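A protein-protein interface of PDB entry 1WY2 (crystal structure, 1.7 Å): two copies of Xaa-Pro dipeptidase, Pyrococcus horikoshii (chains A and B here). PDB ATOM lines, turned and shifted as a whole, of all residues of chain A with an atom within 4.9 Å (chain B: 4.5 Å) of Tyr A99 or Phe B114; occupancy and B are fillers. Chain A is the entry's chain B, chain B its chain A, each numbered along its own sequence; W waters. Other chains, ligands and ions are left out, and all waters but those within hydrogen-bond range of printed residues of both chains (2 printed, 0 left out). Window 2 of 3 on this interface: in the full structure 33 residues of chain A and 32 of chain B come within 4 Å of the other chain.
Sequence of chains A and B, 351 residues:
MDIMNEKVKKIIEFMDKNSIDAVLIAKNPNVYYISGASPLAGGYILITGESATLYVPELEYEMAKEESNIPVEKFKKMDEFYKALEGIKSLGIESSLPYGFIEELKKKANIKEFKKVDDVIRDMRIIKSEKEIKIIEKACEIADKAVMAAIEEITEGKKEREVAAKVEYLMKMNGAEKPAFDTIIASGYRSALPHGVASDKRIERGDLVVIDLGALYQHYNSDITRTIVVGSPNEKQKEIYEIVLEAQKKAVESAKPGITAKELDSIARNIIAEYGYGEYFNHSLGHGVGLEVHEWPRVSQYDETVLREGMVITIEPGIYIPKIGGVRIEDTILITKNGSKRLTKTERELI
O of Leu B97 lies within hydrogen-bond range of N of Tyr A99, at 2.8 Å. N of Gly A100 lies within hydrogen-bond range of O of Ser B95 (2.9 Å). The backbone carbonyl oxygen (O) of Phe B114 is in hydrogen-bond range of the side-chain hydroxyl (OH) of Tyr A99 (3.3 Å). N of Tyr A99 lies within hydrogen-bond range of O of Ser B95 (3.3 Å).
N of Ile B93 is in hydrogen-bond range of O of Lys B115 (2.8 Å).
Pro A98 touches Ser B95 (CB to O, 3.4 Å). Pro A98 touches Leu B97 (CA to O, 3.6 Å). Tyr A99 touches Ile B93. CB of Tyr A99 touches O of Glu B94, 3.9 Å away. CD1 of Tyr A99 touches CD1 of Ile B102, at 3.7 Å. Tyr A99 touches Lys B116. Lys B116 touches Glu A103 (NZ to CG, 3.5 Å).
Of the printed residues of chain B, Tyr A99 touches Ile B93 (3.5 Å), Glu B94 (3.9 Å), Ser B95 (3.3 Å), Leu B97 (2.8 Å), Ile B102 (3.7 Å), Phe B114 (3.3 Å) and Lys B116 (3.5 Å). Of the printed residues of chain B, Gly A100 touches Ser B95 (2.9 Å). Ile A102 touches none of the printed residues of chain B. Printed residues of chain A within 4 Å of Leu B97: Pro A98 (3.6 Å) and Tyr A99 (2.8 Å). Ile B111 touches none of the printed residues of chain A. The nearest printed residue of chain B that does not touch Tyr A99 is Lys B115 (4.03 Å).
Hydrophobic or aromatic side chains of chain A within 4 Å of the printed part of chain B: Pro A98 and Tyr A99. Of the 13 printed residues of chain B, 7 touch a printed residue of chain A. Among the printed residues, no Asp or Glu carboxylate lies within 4 Å of a Lys or Arg side-chain nitrogen of the other chain.
Positions printed for both chains: 97 and 102. Of the 11 pairs that touch across the chains among the printed residues, none has its exchanged pair printed and touching as well.
Water W1 lies within hydrogen-bond range of the backbone NH of Tyr A99 (3.1 Å), the backbone carbonyl oxygen of Leu A97 (3.2 Å) and the backbone carbonyl oxygen of Leu B97 (3.3 Å). Water W2 lies within hydrogen-bond range of O of Ser B95 and N of Phe A101.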
ATOM      1  N   LEU A  97     -22.073  22.727  21.465  1.00  0.00           N
ATOM      2  CA  LEU A  97     -21.932  21.650  20.487  1.00  0.00           C
ATOM      3  C   LEU A  97     -23.209  20.809  20.435  1.00  0.00           C
ATOM      4  O   LEU A  97     -23.672  20.304  21.454  1.00  0.00           O
ATOM      5  CB  LEU A  97     -20.732  20.773  20.839  1.00  0.00           C
ATOM      6  CG  LEU A  97     -20.087  20.031  19.667  1.00  0.00           C
ATOM      7  CD1 LEU A  97     -19.579  21.033  18.636  1.00  0.00           C
ATOM      8  CD2 LEU A  97     -18.944  19.177  20.186  1.00  0.00           C
ATOM      9  N   PRO A  98     -23.788  20.643  19.236  1.00  0.00           N
ATOM     10  CA  PRO A  98     -25.021  19.867  19.057  1.00  0.00           C
ATOM     11  C   PRO A  98     -24.934  18.350  19.217  1.00  0.00           C
ATOM     12  O   PRO A  98     -23.916  17.727  18.926  1.00  0.00           O
ATOM     13  CB  PRO A  98     -25.480  20.280  17.661  1.00  0.00           C
ATOM     14  CG  PRO A  98     -24.193  20.478  16.944  1.00  0.00           C
ATOM     15  CD  PRO A  98     -23.362  21.245  17.960  1.00  0.00           C
ATOM     16  N   TYR A  99     -26.045  17.776  19.671  1.00  0.00           N
ATOM     17  CA  TYR A  99     -26.186  16.344  19.907  1.00  0.00           C
ATOM     18  C   TYR A  99     -25.734  15.470  18.736  1.00  0.00           C
ATOM     19  O   TYR A  99     -24.950  14.535  18.914  1.00  0.00           O
ATOM     20  CB  TYR A  99     -27.651  16.047  20.251  1.00  0.00           C
ATOM     21  CG  TYR A  99     -27.956  14.603  20.569  1.00  0.00           C
ATOM     22  CD1 TYR A  99     -27.310  13.946  21.616  1.00  0.00           C
ATOM     23  CD2 TYR A  99     -28.914  13.896  19.836  1.00  0.00           C
ATOM     24  CE1 TYR A  99     -27.609  12.623  21.931  1.00  0.00           C
ATOM     25  CE2 TYR A  99     -29.221  12.571  20.143  1.00  0.00           C
ATOM     26  CZ  TYR A  99     -28.565  11.942  21.191  1.00  0.00           C
ATOM     27  OH  TYR A  99     -28.868  10.635  21.502  1.00  0.00           O
ATOM     28  N   GLY A 100     -26.235  15.771  17.542  1.00  0.00           N
ATOM     29  CA  GLY A 100     -25.872  14.987  16.375  1.00  0.00           C
ATOM     30  C   GLY A 100     -24.374  14.891  16.168  1.00  0.00           C
ATOM     31  O   GLY A 100     -23.845  13.824  15.851  1.00  0.00           O
ATOM     32  N   PHE A 101     -23.687  16.011  16.363  1.00  0.00           N
ATOM     33  CA  PHE A 101     -22.243  16.063  16.180  1.00  0.00           C
ATOM     34  C   PHE A 101     -21.533  15.251  17.255  1.00  0.00           C
ATOM     35  O   PHE A 101     -20.605  14.497  16.966  1.00  0.00           O
ATOM     36  CB  PHE A 101     -21.774  17.519  16.218  1.00  0.00           C
ATOM     37  CG  PHE A 101     -20.368  17.721  15.731  1.00  0.00           C
ATOM     38  CD1 PHE A 101     -19.963  17.215  14.501  1.00  0.00           C
ATOM     39  CD2 PHE A 101     -19.457  18.446  16.487  1.00  0.00           C
ATOM     40  CE1 PHE A 101     -18.667  17.428  14.030  1.00  0.00           C
ATOM     41  CE2 PHE A 101     -18.161  18.666  16.024  1.00  0.00           C
ATOM     42  CZ  PHE A 101     -17.767  18.156  14.793  1.00  0.00           C
ATOM     43  N   ILE A 102     -21.976  15.407  18.497  1.00  0.00           N
ATOM     44  CA  ILE A 102     -21.384  14.681  19.609  1.00  0.00           C
ATOM     45  C   ILE A 102     -21.528  13.175  19.420  1.00  0.00           C
ATOM     46  O   ILE A 102     -20.603  12.422  19.706  1.00  0.00           O
ATOM     47  CB  ILE A 102     -22.026  15.105  20.945  1.00  0.00           C
ATOM     48  CG1 ILE A 102     -21.692  16.574  21.219  1.00  0.00           C
ATOM     49  CG2 ILE A 102     -21.523  14.217  22.082  1.00  0.00           C
ATOM     50  CD1 ILE A 102     -22.273  17.122  22.502  1.00  0.00           C
ATOM     51  N   GLU A 103     -22.682  12.737  18.928  1.00  0.00           N
ATOM     52  CA  GLU A 103     -22.901  11.313  18.706  1.00  0.00           C
ATOM     53  C   GLU A 103     -21.988  10.791  17.603  1.00  0.00           C
ATOM     54  O   GLU A 103     -21.517   9.660  17.669  1.00  0.00           O
ATOM     55  CB  GLU A 103     -24.369  11.046  18.367  1.00  0.00           C
ATOM     56  CG  GLU A 103     -25.293  11.224  19.563  1.00  0.00           C
ATOM     57  CD  GLU A 103     -24.928  10.301  20.715  1.00  0.00           C
ATOM     58  OE1 GLU A 103     -24.968   9.069  20.522  1.00  0.00           O
ATOM     59  OE2 GLU A 103     -24.597  10.802  21.811  1.00  0.00           O
ATOM     60  N   LEU B  91     -35.974  10.128  26.346  1.00  0.00           N
ATOM     61  CA  LEU B  91     -36.405  11.385  25.737  1.00  0.00           C
ATOM     62  C   LEU B  91     -35.914  11.543  24.300  1.00  0.00           C
ATOM     63  O   LEU B  91     -34.724  11.403  24.027  1.00  0.00           O
ATOM     64  CB  LEU B  91     -35.895  12.573  26.564  1.00  0.00           C
ATOM     65  CG  LEU B  91     -36.284  13.980  26.094  1.00  0.00           C
ATOM     66  CD1 LEU B  91     -37.771  14.219  26.360  1.00  0.00           C
ATOM     67  CD2 LEU B  91     -35.451  15.023  26.822  1.00  0.00           C
ATOM     68  N   ILE B  93     -34.921  13.729  21.161  1.00  0.00           N
ATOM     69  CA  ILE B  93     -34.441  15.095  20.962  1.00  0.00           C
ATOM     70  C   ILE B  93     -33.920  15.370  19.553  1.00  0.00           C
ATOM     71  O   ILE B  93     -33.622  14.449  18.793  1.00  0.00           O
ATOM     72  CB  ILE B  93     -33.307  15.451  21.961  1.00  0.00           C
ATOM     73  CG1 ILE B  93     -32.122  14.498  21.773  1.00  0.00           C
ATOM     74  CG2 ILE B  93     -33.826  15.374  23.396  1.00  0.00           C
ATOM     75  CD1 ILE B  93     -30.864  14.937  22.521  1.00  0.00           C
ATOM     76  N   GLU B  94     -33.821  16.655  19.218  1.00  0.00           N
ATOM     77  CA  GLU B  94     -33.323  17.087  17.912  1.00  0.00           C
ATOM     78  C   GLU B  94     -31.801  16.983  17.882  1.00  0.00           C
ATOM     79  O   GLU B  94     -31.141  17.126  18.910  1.00  0.00           O
ATOM     80  CB  GLU B  94     -33.709  18.540  17.653  1.00  0.00           C
ATOM     81  CG  GLU B  94     -35.197  18.823  17.679  1.00  0.00           C
ATOM     82  CD  GLU B  94     -35.489  20.242  18.119  1.00  0.00           C
ATOM     83  OE1 GLU B  94     -35.107  20.599  19.258  1.00  0.00           O
ATOM     84  OE2 GLU B  94     -36.096  21.003  17.338  1.00  0.00           O
ATOM     85  N   SER B  95     -31.248  16.756  16.699  1.00  0.00           N
ATOM     86  CA  SER B  95     -29.801  16.644  16.557  1.00  0.00           C
ATOM     87  C   SER B  95     -29.114  17.978  16.829  1.00  0.00           C
ATOM     88  O   SER B  95     -27.891  18.039  16.955  1.00  0.00           O
ATOM     89  CB  SER B  95     -29.448  16.159  15.152  1.00  0.00           C
ATOM     90  OG  SER B  95     -29.931  14.844  14.937  1.00  0.00           O
ATOM     91  N   LEU B  97     -29.896  19.934  19.527  1.00  0.00           N
ATOM     92  CA  LEU B  97     -29.896  20.246  20.956  1.00  0.00           C
ATOM     93  C   LEU B  97     -28.463  20.301  21.480  1.00  0.00           C
ATOM     94  O   LEU B  97     -27.706  19.341  21.345  1.00  0.00           O
ATOM     95  CB  LEU B  97     -30.705  19.207  21.734  1.00  0.00           C
ATOM     96  CG  LEU B  97     -31.270  19.732  23.057  1.00  0.00           C
ATOM     97  CD1 LEU B  97     -32.229  20.885  22.775  1.00  0.00           C
ATOM     98  CD2 LEU B  97     -31.982  18.609  23.800  1.00  0.00           C
ATOM     99  N   ILE B 102     -28.384  19.378  27.362  1.00  0.00           N
ATOM    100  CA  ILE B 102     -28.565  17.948  27.580  1.00  0.00           C
ATOM    101  C   ILE B 102     -28.027  17.527  28.944  1.00  0.00           C
ATOM    102  O   ILE B 102     -28.609  16.671  29.611  1.00  0.00           O
ATOM    103  CB  ILE B 102     -27.863  17.124  26.486  1.00  0.00           C
ATOM    104  CG1 ILE B 102     -28.559  17.362  25.141  1.00  0.00           C
ATOM    105  CG2 ILE B 102     -27.878  15.648  26.854  1.00  0.00           C
ATOM    106  CD1 ILE B 102     -27.902  16.672  23.974  1.00  0.00           C
ATOM    107  N   LEU B 105     -30.609  18.377  31.509  1.00  0.00           N
ATOM    108  CA  LEU B 105     -31.703  17.411  31.489  1.00  0.00           C
ATOM    109  C   LEU B 105     -31.324  16.132  32.232  1.00  0.00           C
ATOM    110  O   LEU B 105     -32.151  15.538  32.923  1.00  0.00           O
ATOM    111  CB  LEU B 105     -32.081  17.082  30.040  1.00  0.00           C
ATOM    112  CG  LEU B 105     -32.648  18.232  29.202  1.00  0.00           C
ATOM    113  CD1 LEU B 105     -32.735  17.813  27.741  1.00  0.00           C
ATOM    114  CD2 LEU B 105     -34.018  18.626  29.727  1.00  0.00           C
ATOM    115  N   LYS B 106     -30.072  15.714  32.087  1.00  0.00           N
ATOM    116  CA  LYS B 106     -29.588  14.507  32.745  1.00  0.00           C
ATOM    117  C   LYS B 106     -29.597  14.632  34.264  1.00  0.00           C
ATOM    118  O   LYS B 106     -29.950  13.687  34.975  1.00  0.00           O
ATOM    119  CB  LYS B 106     -28.159  14.186  32.297  1.00  0.00           C
ATOM    120  CG  LYS B 106     -28.024  13.703  30.866  1.00  0.00           C
ATOM    121  CD  LYS B 106     -26.578  13.326  30.569  1.00  0.00           C
ATOM    122  CE  LYS B 106     -26.407  12.799  29.156  1.00  0.00           C
ATOM    123  NZ  LYS B 106     -24.988  12.428  28.884  1.00  0.00           N
ATOM    124  N   ILE B 111     -33.141  12.495  33.209  1.00  0.00           N
ATOM    125  CA  ILE B 111     -33.384  11.745  31.983  1.00  0.00           C
ATOM    126  C   ILE B 111     -32.333  10.647  31.864  1.00  0.00           C
ATOM    127  O   ILE B 111     -31.137  10.903  31.991  1.00  0.00           O
ATOM    128  CB  ILE B 111     -33.310  12.655  30.737  1.00  0.00           C
ATOM    129  CG1 ILE B 111     -34.330  13.789  30.858  1.00  0.00           C
ATOM    130  CG2 ILE B 111     -33.566  11.836  29.476  1.00  0.00           C
ATOM    131  CD1 ILE B 111     -35.764  13.321  31.015  1.00  0.00           C
ATOM    132  N   GLU B 113     -32.135   8.128  29.090  1.00  0.00           N
ATOM    133  CA  GLU B 113     -31.683   7.874  27.729  1.00  0.00           C
ATOM    134  C   GLU B 113     -32.188   8.927  26.750  1.00  0.00           C
ATOM    135  O   GLU B 113     -33.269   9.483  26.928  1.00  0.00           O
ATOM    136  CB  GLU B 113     -32.177   6.486  27.299  1.00  0.00           C
ATOM    137  CG  GLU B 113     -31.677   5.995  25.950  1.00  0.00           C
ATOM    138  CD  GLU B 113     -32.240   4.625  25.583  1.00  0.00           C
ATOM    139  OE1 GLU B 113     -32.022   3.657  26.344  1.00  0.00           O
ATOM    140  OE2 GLU B 113     -32.905   4.514  24.532  1.00  0.00           O
ATOM    141  N   PHE B 114     -31.390   9.202  25.722  1.00  0.00           N
ATOM    142  CA  PHE B 114     -31.773  10.160  24.690  1.00  0.00           C
ATOM    143  C   PHE B 114     -31.740   9.455  23.343  1.00  0.00           C
ATOM    144  O   PHE B 114     -30.883   8.605  23.098  1.00  0.00           O
ATOM    145  CB  PHE B 114     -30.811  11.355  24.645  1.00  0.00           C
ATOM    146  CG  PHE B 114     -30.799  12.179  25.896  1.00  0.00           C
ATOM    147  CD1 PHE B 114     -29.980  11.829  26.969  1.00  0.00           C
ATOM    148  CD2 PHE B 114     -31.604  13.304  26.007  1.00  0.00           C
ATOM    149  CE1 PHE B 114     -29.967  12.594  28.135  1.00  0.00           C
ATOM    150  CE2 PHE B 114     -31.601  14.076  27.166  1.00  0.00           C
ATOM    151  CZ  PHE B 114     -30.778  13.720  28.234  1.00  0.00           C
ATOM    152  N   LYS B 115     -32.685   9.799  22.473  1.00  0.00           N
ATOM    153  CA  LYS B 115     -32.748   9.215  21.142  1.00  0.00           C
ATOM    154  C   LYS B 115     -33.044  10.315  20.135  1.00  0.00           C
ATOM    155  O   LYS B 115     -33.715  11.293  20.457  1.00  0.00           O
ATOM    156  CB  LYS B 115     -33.831   8.134  21.064  1.00  0.00           C
ATOM    157  CG  LYS B 115     -33.419   6.791  21.657  1.00  0.00           C
ATOM    158  CD  LYS B 115     -34.374   5.689  21.223  1.00  0.00           C
ATOM    159  CE  LYS B 115     -33.862   4.316  21.631  1.00  0.00           C
ATOM    160  NZ  LYS B 115     -34.724   3.224  21.094  1.00  0.00           N
ATOM    161  N   LYS B 116     -32.530  10.157  18.921  1.00  0.00           N
ATOM    162  CA  LYS B 116     -32.740  11.149  17.872  1.00  0.00           C
ATOM    163  C   LYS B 116     -34.138  11.043  17.274  1.00  0.00           C
ATOM    164  O   LYS B 116     -34.640   9.941  17.053  1.00  0.00           O
ATOM    165  CB  LYS B 116     -31.726  10.952  16.740  1.00  0.00           C
ATOM    166  CG  LYS B 116     -30.268  11.097  17.134  1.00  0.00           C
ATOM    167  CD  LYS B 116     -29.369  10.894  15.920  1.00  0.00           C
ATOM    168  CE  LYS B 116     -27.899  10.948  16.297  1.00  0.00           C
ATOM    169  NZ  LYS B 116     -27.534   9.877  17.265  1.00  0.00           N
HETATM  170  O   HOH W   1     -25.185  17.727  22.647  1.00  0.00           O
HETATM  171  O   HOH W   2     -25.647  17.990  14.791  1.00  0.00           O
